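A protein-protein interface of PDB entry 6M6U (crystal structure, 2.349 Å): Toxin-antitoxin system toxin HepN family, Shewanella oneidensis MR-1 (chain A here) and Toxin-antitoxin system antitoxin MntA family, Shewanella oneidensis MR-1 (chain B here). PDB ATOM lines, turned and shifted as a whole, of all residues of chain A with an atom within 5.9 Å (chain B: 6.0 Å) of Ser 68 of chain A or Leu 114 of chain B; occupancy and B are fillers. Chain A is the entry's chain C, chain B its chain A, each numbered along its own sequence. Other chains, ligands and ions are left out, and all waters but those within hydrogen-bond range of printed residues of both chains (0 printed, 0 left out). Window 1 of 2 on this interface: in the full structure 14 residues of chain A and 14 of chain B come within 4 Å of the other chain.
The side-chain carboxylate (OE1) of Glu 117 of chain B lies within hydrogen-bond range of the side-chain hydroxyl (OG) of Ser 69 of chain A (2.6 Å).
The guanidinium group of Arg 118 of chain B sits at hydrogen-bond distance from the backbone carbonyl oxygen of Pro 66 of chain A (2.9 Å).
The backbone NH (N) of Val 81 of chain B is in hydrogen-bond range of the backbone carbonyl oxygen (O) of Gln 67 of chain A (3.0 Å).
O of Gln 67 of chain A is in hydrogen-bond range of N of Thr 80 of chain B, at 3.2 Å.
The side-chain hydroxyl (OG) of Ser 68 of chain A lies within hydrogen-bond range of the backbone NH (N) of Asp 71 of chain A, at 3.4 Å.
The side-chain amide oxygen (OE1) of Gln 115 of chain B is in hydrogen-bond range of the guanidinium group (NE) of Arg 118 of chain B, at 2.6 Å.
The side-chain carboxylate (OD2) of Asp 71 of chain A lies within hydrogen-bond range of the backbone NH (N) of Gln 67 of chain A (3.0 Å).
The backbone NH of Val 81 of chain B sits close to the side-chain hydroxyl of Ser 79 of chain B (3.4 Å).
Among the printed residues, pairs that only touch across the chains: Ser 68 of chain A with Thr 80 of chain B (3.1 Å), Gln 67 of chain A with Leu 114 of chain B (3.5 Å), Gln 67 of chain A with Ser 79 of chain B (3.6 Å), Ser 68 of chain A with Leu 114 of chain B (3.6 Å) and Ser 69 of chain A with Leu 114 of chain B (3.8 Å).
Ser 68 of chain A touches just these residues of chain B: Thr 80 and Leu 114.
Of chain A, only Gln 67 (3.5 Å), Ser 68 (3.6 Å) and Ser 69 (3.8 Å) come within 4 Å of Leu 114 of chain B.
Of the printed residues of chain A, Val 81 of chain B touches Gln 67 (3.0 Å).
Printed residues of chain B within 4 Å of Ser 69 of chain A: Leu 114 (3.8 Å) and Glu 117 (2.6 Å).
Of the printed residues of chain A, Ser 79 of chain B touches Gln 67.
Printed residues of chain A within 4 Å of Arg 118 of chain B: Pro 66.
Of the printed residues of chain A, Thr 80 of chain B touches Gln 67 and Ser 68.
His 113 of chain B touches none of the printed residues of chain A.
Gln 119 of chain B touches none of the printed residues of chain A.
The nearest residue of chain B that does not touch Ser 68 of chain A is Ser 79 of chain B (4.6 Å).
The nearest residue of chain A that does not touch Leu 114 of chain B is Pro 66 of chain A (4.3 Å).
Of the 15 printed residues of chain B, 6 touch a printed residue of chain A.
Hydrophobic or aromatic side chains of chain B that line the printed part of chain A: Val 81 and Leu 114.
Along chain B the printed residues that touch a printed residue of chain A span positions 79 to 118.
Of the 7 printed residues of chain A, 4 touch a printed residue of chain B.
Hydrophobic or aromatic side chains of chain A that line the printed part of chain B: Pro 66.
Among the printed residues, 9 pairs touch across the chains.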
ATOM      1  N   PRO A  66     -33.671 -21.453  -7.025  1.00  0.00           N
ATOM      2  CA  PRO A  66     -33.213 -20.077  -6.811  1.00  0.00           C
ATOM      3  C   PRO A  66     -32.299 -19.633  -7.943  1.00  0.00           C
ATOM      4  O   PRO A  66     -31.447 -20.389  -8.412  1.00  0.00           O
ATOM      5  CB  PRO A  66     -32.468 -20.148  -5.467  1.00  0.00           C
ATOM      6  CG  PRO A  66     -32.154 -21.586  -5.264  1.00  0.00           C
ATOM      7  CD  PRO A  66     -33.262 -22.354  -5.935  1.00  0.00           C
ATOM      8  N   GLN A  67     -32.512 -18.402  -8.400  1.00  0.00           N
ATOM      9  CA  GLN A  67     -31.730 -17.816  -9.483  1.00  0.00           C
ATOM     10  C   GLN A  67     -30.646 -16.887  -8.962  1.00  0.00           C
ATOM     11  O   GLN A  67     -29.823 -16.403  -9.749  1.00  0.00           O
ATOM     12  CB  GLN A  67     -32.650 -17.048 -10.450  1.00  0.00           C
ATOM     13  CG  GLN A  67     -33.806 -17.883 -10.991  1.00  0.00           C
ATOM     14  CD  GLN A  67     -33.331 -19.003 -11.897  1.00  0.00           C
ATOM     15  OE1 GLN A  67     -32.782 -18.753 -12.972  1.00  0.00           O
ATOM     16  NE2 GLN A  67     -33.522 -20.248 -11.458  1.00  0.00           N
ATOM     17  N   SER A  68     -30.654 -16.624  -7.661  1.00  0.00           N
ATOM     18  CA  SER A  68     -29.610 -15.894  -6.964  1.00  0.00           C
ATOM     19  C   SER A  68     -29.740 -16.275  -5.499  1.00  0.00           C
ATOM     20  O   SER A  68     -30.694 -16.954  -5.103  1.00  0.00           O
ATOM     21  CB  SER A  68     -29.744 -14.382  -7.158  1.00  0.00           C
ATOM     22  OG  SER A  68     -30.826 -13.888  -6.388  1.00  0.00           O
ATOM     23  N   SER A  69     -28.774 -15.833  -4.692  1.00  0.00           N
ATOM     24  CA  SER A  69     -28.802 -16.185  -3.276  1.00  0.00           C
ATOM     25  C   SER A  69     -30.016 -15.588  -2.574  1.00  0.00           C
ATOM     26  O   SER A  69     -30.623 -16.243  -1.719  1.00  0.00           O
ATOM     27  CB  SER A  69     -27.508 -15.742  -2.593  1.00  0.00           C
ATOM     28  OG  SER A  69     -26.436 -16.599  -2.960  1.00  0.00           O
ATOM     29  N   ARG A  70     -30.384 -14.346  -2.913  1.00  0.00           N
ATOM     30  CA  ARG A  70     -31.573 -13.744  -2.315  1.00  0.00           C
ATOM     31  C   ARG A  70     -32.824 -14.521  -2.677  1.00  0.00           C
ATOM     32  O   ARG A  70     -33.723 -14.687  -1.844  1.00  0.00           O
ATOM     33  CB  ARG A  70     -31.736 -12.302  -2.766  1.00  0.00           C
ATOM     34  CG  ARG A  70     -30.548 -11.453  -2.556  1.00  0.00           C
ATOM     35  CD  ARG A  70     -31.020 -10.075  -2.197  1.00  0.00           C
ATOM     36  NE  ARG A  70     -29.903  -9.184  -1.904  1.00  0.00           N
ATOM     37  CZ  ARG A  70     -29.020  -8.791  -2.819  1.00  0.00           C
ATOM     38  NH1 ARG A  70     -29.136  -9.219  -4.063  1.00  0.00           N
ATOM     39  NH2 ARG A  70     -28.054  -7.966  -2.483  1.00  0.00           N
ATOM     40  N   ASP A  71     -32.903 -14.989  -3.923  1.00  0.00           N
ATOM     41  CA  ASP A  71     -34.081 -15.706  -4.386  1.00  0.00           C
ATOM     42  C   ASP A  71     -34.420 -16.873  -3.473  1.00  0.00           C
ATOM     43  O   ASP A  71     -35.582 -17.297  -3.421  1.00  0.00           O
ATOM     44  CB  ASP A  71     -33.848 -16.183  -5.819  1.00  0.00           C
ATOM     45  CG  ASP A  71     -35.131 -16.471  -6.549  1.00  0.00           C
ATOM     46  OD1 ASP A  71     -36.120 -15.739  -6.318  1.00  0.00           O
ATOM     47  OD2 ASP A  71     -35.153 -17.430  -7.350  1.00  0.00           O
ATOM     48  N   SER A  72     -33.434 -17.373  -2.729  1.00  0.00           N
ATOM     49  CA  SER A  72     -33.670 -18.456  -1.785  1.00  0.00           C
ATOM     50  C   SER A  72     -34.679 -18.049  -0.715  1.00  0.00           C
ATOM     51  O   SER A  72     -35.511 -18.861  -0.290  1.00  0.00           O
ATOM     52  CB  SER A  72     -32.341 -18.870  -1.160  1.00  0.00           C
ATOM     53  OG  SER A  72     -32.371 -20.220  -0.752  1.00  0.00           O
ATOM     54  N   ALA B  78     -31.149  -7.812 -12.199  1.00  0.00           N
ATOM     55  CA  ALA B  78     -31.373  -9.126 -12.780  1.00  0.00           C
ATOM     56  C   ALA B  78     -30.764 -10.212 -11.901  1.00  0.00           C
ATOM     57  O   ALA B  78     -29.818  -9.983 -11.144  1.00  0.00           O
ATOM     58  CB  ALA B  78     -30.789  -9.200 -14.190  1.00  0.00           C
ATOM     59  N   SER B  79     -31.317 -11.414 -12.021  1.00  0.00           N
ATOM     60  CA  SER B  79     -30.840 -12.536 -11.232  1.00  0.00           C
ATOM     61  C   SER B  79     -29.386 -12.870 -11.574  1.00  0.00           C
ATOM     62  O   SER B  79     -28.868 -12.527 -12.645  1.00  0.00           O
ATOM     63  CB  SER B  79     -31.714 -13.762 -11.478  1.00  0.00           C
ATOM     64  OG  SER B  79     -31.309 -14.390 -12.675  1.00  0.00           O
ATOM     65  N   THR B  80     -28.731 -13.568 -10.644  1.00  0.00           N
ATOM     66  CA  THR B  80     -27.356 -13.994 -10.876  1.00  0.00           C
ATOM     67  C   THR B  80     -27.265 -14.958 -12.051  1.00  0.00           C
ATOM     68  O   THR B  80     -26.301 -14.914 -12.822  1.00  0.00           O
ATOM     69  CB  THR B  80     -26.798 -14.642  -9.615  1.00  0.00           C
ATOM     70  OG1 THR B  80     -26.980 -13.739  -8.523  1.00  0.00           O
ATOM     71  CG2 THR B  80     -25.319 -14.951  -9.780  1.00  0.00           C
ATOM     72  N   VAL B  81     -28.264 -15.833 -12.209  1.00  0.00           N
ATOM     73  CA  VAL B  81     -28.281 -16.752 -13.349  1.00  0.00           C
ATOM     74  C   VAL B  81     -28.297 -15.977 -14.661  1.00  0.00           C
ATOM     75  O   VAL B  81     -27.512 -16.255 -15.577  1.00  0.00           O
ATOM     76  CB  VAL B  81     -29.477 -17.715 -13.246  1.00  0.00           C
ATOM     77  CG1 VAL B  81     -29.763 -18.369 -14.597  1.00  0.00           C
ATOM     78  CG2 VAL B  81     -29.203 -18.772 -12.187  1.00  0.00           C
ATOM     79  N   SER B 109     -18.179 -14.766  -9.862  1.00  0.00           N
ATOM     80  CA  SER B 109     -17.980 -15.130  -8.463  1.00  0.00           C
ATOM     81  C   SER B 109     -19.311 -15.405  -7.772  1.00  0.00           C
ATOM     82  O   SER B 109     -19.482 -16.444  -7.120  1.00  0.00           O
ATOM     83  CB  SER B 109     -17.213 -14.022  -7.742  1.00  0.00           C
ATOM     84  OG  SER B 109     -17.095 -14.312  -6.362  1.00  0.00           O
ATOM     85  N   MET B 110     -20.263 -14.479  -7.900  1.00  0.00           N
ATOM     86  CA  MET B 110     -21.593 -14.692  -7.333  1.00  0.00           C
ATOM     87  C   MET B 110     -22.219 -15.981  -7.849  1.00  0.00           C
ATOM     88  O   MET B 110     -22.863 -16.716  -7.090  1.00  0.00           O
ATOM     89  CB  MET B 110     -22.498 -13.498  -7.646  1.00  0.00           C
ATOM     90  CG  MET B 110     -22.073 -12.212  -6.955  1.00  0.00           C
ATOM     91  SD  MET B 110     -23.259 -10.865  -7.142  1.00  0.00           S
ATOM     92  CE  MET B 110     -24.586 -11.445  -6.085  1.00  0.00           C
ATOM     93  N   TYR B 111     -22.024 -16.283  -9.135  1.00  0.00           N
ATOM     94  CA  TYR B 111     -22.628 -17.481  -9.710  1.00  0.00           C
ATOM     95  C   TYR B 111     -22.022 -18.742  -9.109  1.00  0.00           C
ATOM     96  O   TYR B 111     -22.750 -19.668  -8.731  1.00  0.00           O
ATOM     97  CB  TYR B 111     -22.473 -17.483 -11.231  1.00  0.00           C
ATOM     98  CG  TYR B 111     -23.203 -18.627 -11.906  1.00  0.00           C
ATOM     99  CD1 TYR B 111     -22.525 -19.777 -12.299  1.00  0.00           C
ATOM    100  CD2 TYR B 111     -24.575 -18.561 -12.131  1.00  0.00           C
ATOM    101  CE1 TYR B 111     -23.181 -20.815 -12.907  1.00  0.00           C
ATOM    102  CE2 TYR B 111     -25.250 -19.601 -12.738  1.00  0.00           C
ATOM    103  CZ  TYR B 111     -24.549 -20.724 -13.128  1.00  0.00           C
ATOM    104  OH  TYR B 111     -25.219 -21.762 -13.731  1.00  0.00           O
ATOM    105  N   GLN B 112     -20.689 -18.795  -9.013  1.00  0.00           N
ATOM    106  CA  GLN B 112     -20.032 -19.958  -8.417  1.00  0.00           C
ATOM    107  C   GLN B 112     -20.501 -20.188  -6.984  1.00  0.00           C
ATOM    108  O   GLN B 112     -20.781 -21.327  -6.591  1.00  0.00           O
ATOM    109  CB  GLN B 112     -18.516 -19.789  -8.470  1.00  0.00           C
ATOM    110  CG  GLN B 112     -17.951 -19.938  -9.866  1.00  0.00           C
ATOM    111  CD  GLN B 112     -16.542 -19.413  -9.980  1.00  0.00           C
ATOM    112  OE1 GLN B 112     -16.031 -18.765  -9.065  1.00  0.00           O
ATOM    113  NE2 GLN B 112     -15.901 -19.683 -11.113  1.00  0.00           N
ATOM    114  N   HIS B 113     -20.608 -19.120  -6.190  1.00  0.00           N
ATOM    115  CA  HIS B 113     -21.152 -19.269  -4.843  1.00  0.00           C
ATOM    116  C   HIS B 113     -22.611 -19.704  -4.872  1.00  0.00           C
ATOM    117  O   HIS B 113     -23.047 -20.465  -4.001  1.00  0.00           O
ATOM    118  CB  HIS B 113     -21.005 -17.966  -4.064  1.00  0.00           C
ATOM    119  CG  HIS B 113     -19.605 -17.691  -3.617  1.00  0.00           C
ATOM    120  ND1 HIS B 113     -19.159 -17.989  -2.346  1.00  0.00           N
ATOM    121  CD2 HIS B 113     -18.547 -17.153  -4.272  1.00  0.00           C
ATOM    122  CE1 HIS B 113     -17.889 -17.642  -2.236  1.00  0.00           C
ATOM    123  NE2 HIS B 113     -17.494 -17.132  -3.391  1.00  0.00           N
ATOM    124  N   LEU B 114     -23.382 -19.237  -5.858  1.00  0.00           N
ATOM    125  CA  LEU B 114     -24.765 -19.686  -5.963  1.00  0.00           C
ATOM    126  C   LEU B 114     -24.835 -21.172  -6.295  1.00  0.00           C
ATOM    127  O   LEU B 114     -25.633 -21.906  -5.701  1.00  0.00           O
ATOM    128  CB  LEU B 114     -25.513 -18.866  -7.012  1.00  0.00           C
ATOM    129  CG  LEU B 114     -26.920 -19.394  -7.303  1.00  0.00           C
ATOM    130  CD1 LEU B 114     -27.821 -19.231  -6.079  1.00  0.00           C
ATOM    131  CD2 LEU B 114     -27.516 -18.707  -8.523  1.00  0.00           C
ATOM    132  N   GLN B 115     -24.000 -21.635  -7.231  1.00  0.00           N
ATOM    133  CA  GLN B 115     -24.026 -23.045  -7.608  1.00  0.00           C
ATOM    134  C   GLN B 115     -23.775 -23.948  -6.407  1.00  0.00           C
ATOM    135  O   GLN B 115     -24.395 -25.010  -6.284  1.00  0.00           O
ATOM    136  CB  GLN B 115     -23.002 -23.317  -8.711  1.00  0.00           C
ATOM    137  CG  GLN B 115     -23.405 -22.793 -10.090  1.00  0.00           C
ATOM    138  CD  GLN B 115     -24.611 -23.525 -10.688  1.00  0.00           C
ATOM    139  OE1 GLN B 115     -25.734 -23.434 -10.176  1.00  0.00           O
ATOM    140  NE2 GLN B 115     -24.377 -24.256 -11.774  1.00  0.00           N
ATOM    141  N   ALA B 116     -22.884 -23.538  -5.501  1.00  0.00           N
ATOM    142  CA  ALA B 116     -22.647 -24.318  -4.290  1.00  0.00           C
ATOM    143  C   ALA B 116     -23.904 -24.390  -3.426  1.00  0.00           C
ATOM    144  O   ALA B 116     -24.307 -25.475  -2.989  1.00  0.00           O
ATOM    145  CB  ALA B 116     -21.481 -23.726  -3.499  1.00  0.00           C
ATOM    146  N   GLU B 117     -24.543 -23.242  -3.177  1.00  0.00           N
ATOM    147  CA  GLU B 117     -25.707 -23.218  -2.295  1.00  0.00           C
ATOM    148  C   GLU B 117     -26.849 -24.067  -2.839  1.00  0.00           C
ATOM    149  O   GLU B 117     -27.534 -24.756  -2.075  1.00  0.00           O
ATOM    150  CB  GLU B 117     -26.191 -21.781  -2.082  1.00  0.00           C
ATOM    151  CG  GLU B 117     -25.101 -20.799  -1.711  1.00  0.00           C
ATOM    152  CD  GLU B 117     -25.568 -19.357  -1.752  1.00  0.00           C
ATOM    153  OE1 GLU B 117     -26.670 -19.094  -2.285  1.00  0.00           O
ATOM    154  OE2 GLU B 117     -24.817 -18.483  -1.258  1.00  0.00           O
ATOM    155  N   ARG B 118     -27.066 -24.038  -4.153  1.00  0.00           N
ATOM    156  CA  ARG B 118     -28.292 -24.543  -4.751  1.00  0.00           C
ATOM    157  C   ARG B 118     -28.130 -25.880  -5.470  1.00  0.00           C
ATOM    158  O   ARG B 118     -29.111 -26.370  -6.045  1.00  0.00           O
ATOM    159  CB  ARG B 118     -28.850 -23.504  -5.733  1.00  0.00           C
ATOM    160  CG  ARG B 118     -28.028 -23.373  -7.011  1.00  0.00           C
ATOM    161  CD  ARG B 118     -28.722 -22.502  -8.035  1.00  0.00           C
ATOM    162  NE  ARG B 118     -28.051 -22.542  -9.330  1.00  0.00           N
ATOM    163  CZ  ARG B 118     -28.633 -22.186 -10.471  1.00  0.00           C
ATOM    164  NH1 ARG B 118     -29.890 -21.769 -10.463  1.00  0.00           N
ATOM    165  NH2 ARG B 118     -27.966 -22.252 -11.616  1.00  0.00           N
ATOM    166  N   GLN B 119     -26.941 -26.496  -5.453  1.00  0.00           N
ATOM    167  CA  GLN B 119     -26.708 -27.666  -6.305  1.00  0.00           C
ATOM    168  C   GLN B 119     -27.515 -28.877  -5.849  1.00  0.00           C
ATOM    169  O   GLN B 119     -27.830 -29.748  -6.668  1.00  0.00           O
ATOM    170  CB  GLN B 119     -25.216 -28.016  -6.369  1.00  0.00           C
ATOM    171  CG  GLN B 119     -24.822 -28.983  -7.500  1.00  0.00           C
ATOM    172  CD  GLN B 119     -24.811 -28.314  -8.882  1.00  0.00           C
ATOM    173  OE1 GLN B 119     -24.799 -27.082  -8.984  1.00  0.00           O
ATOM    174  NE2 GLN B 119     -24.803 -29.137  -9.944  1.00  0.00           N
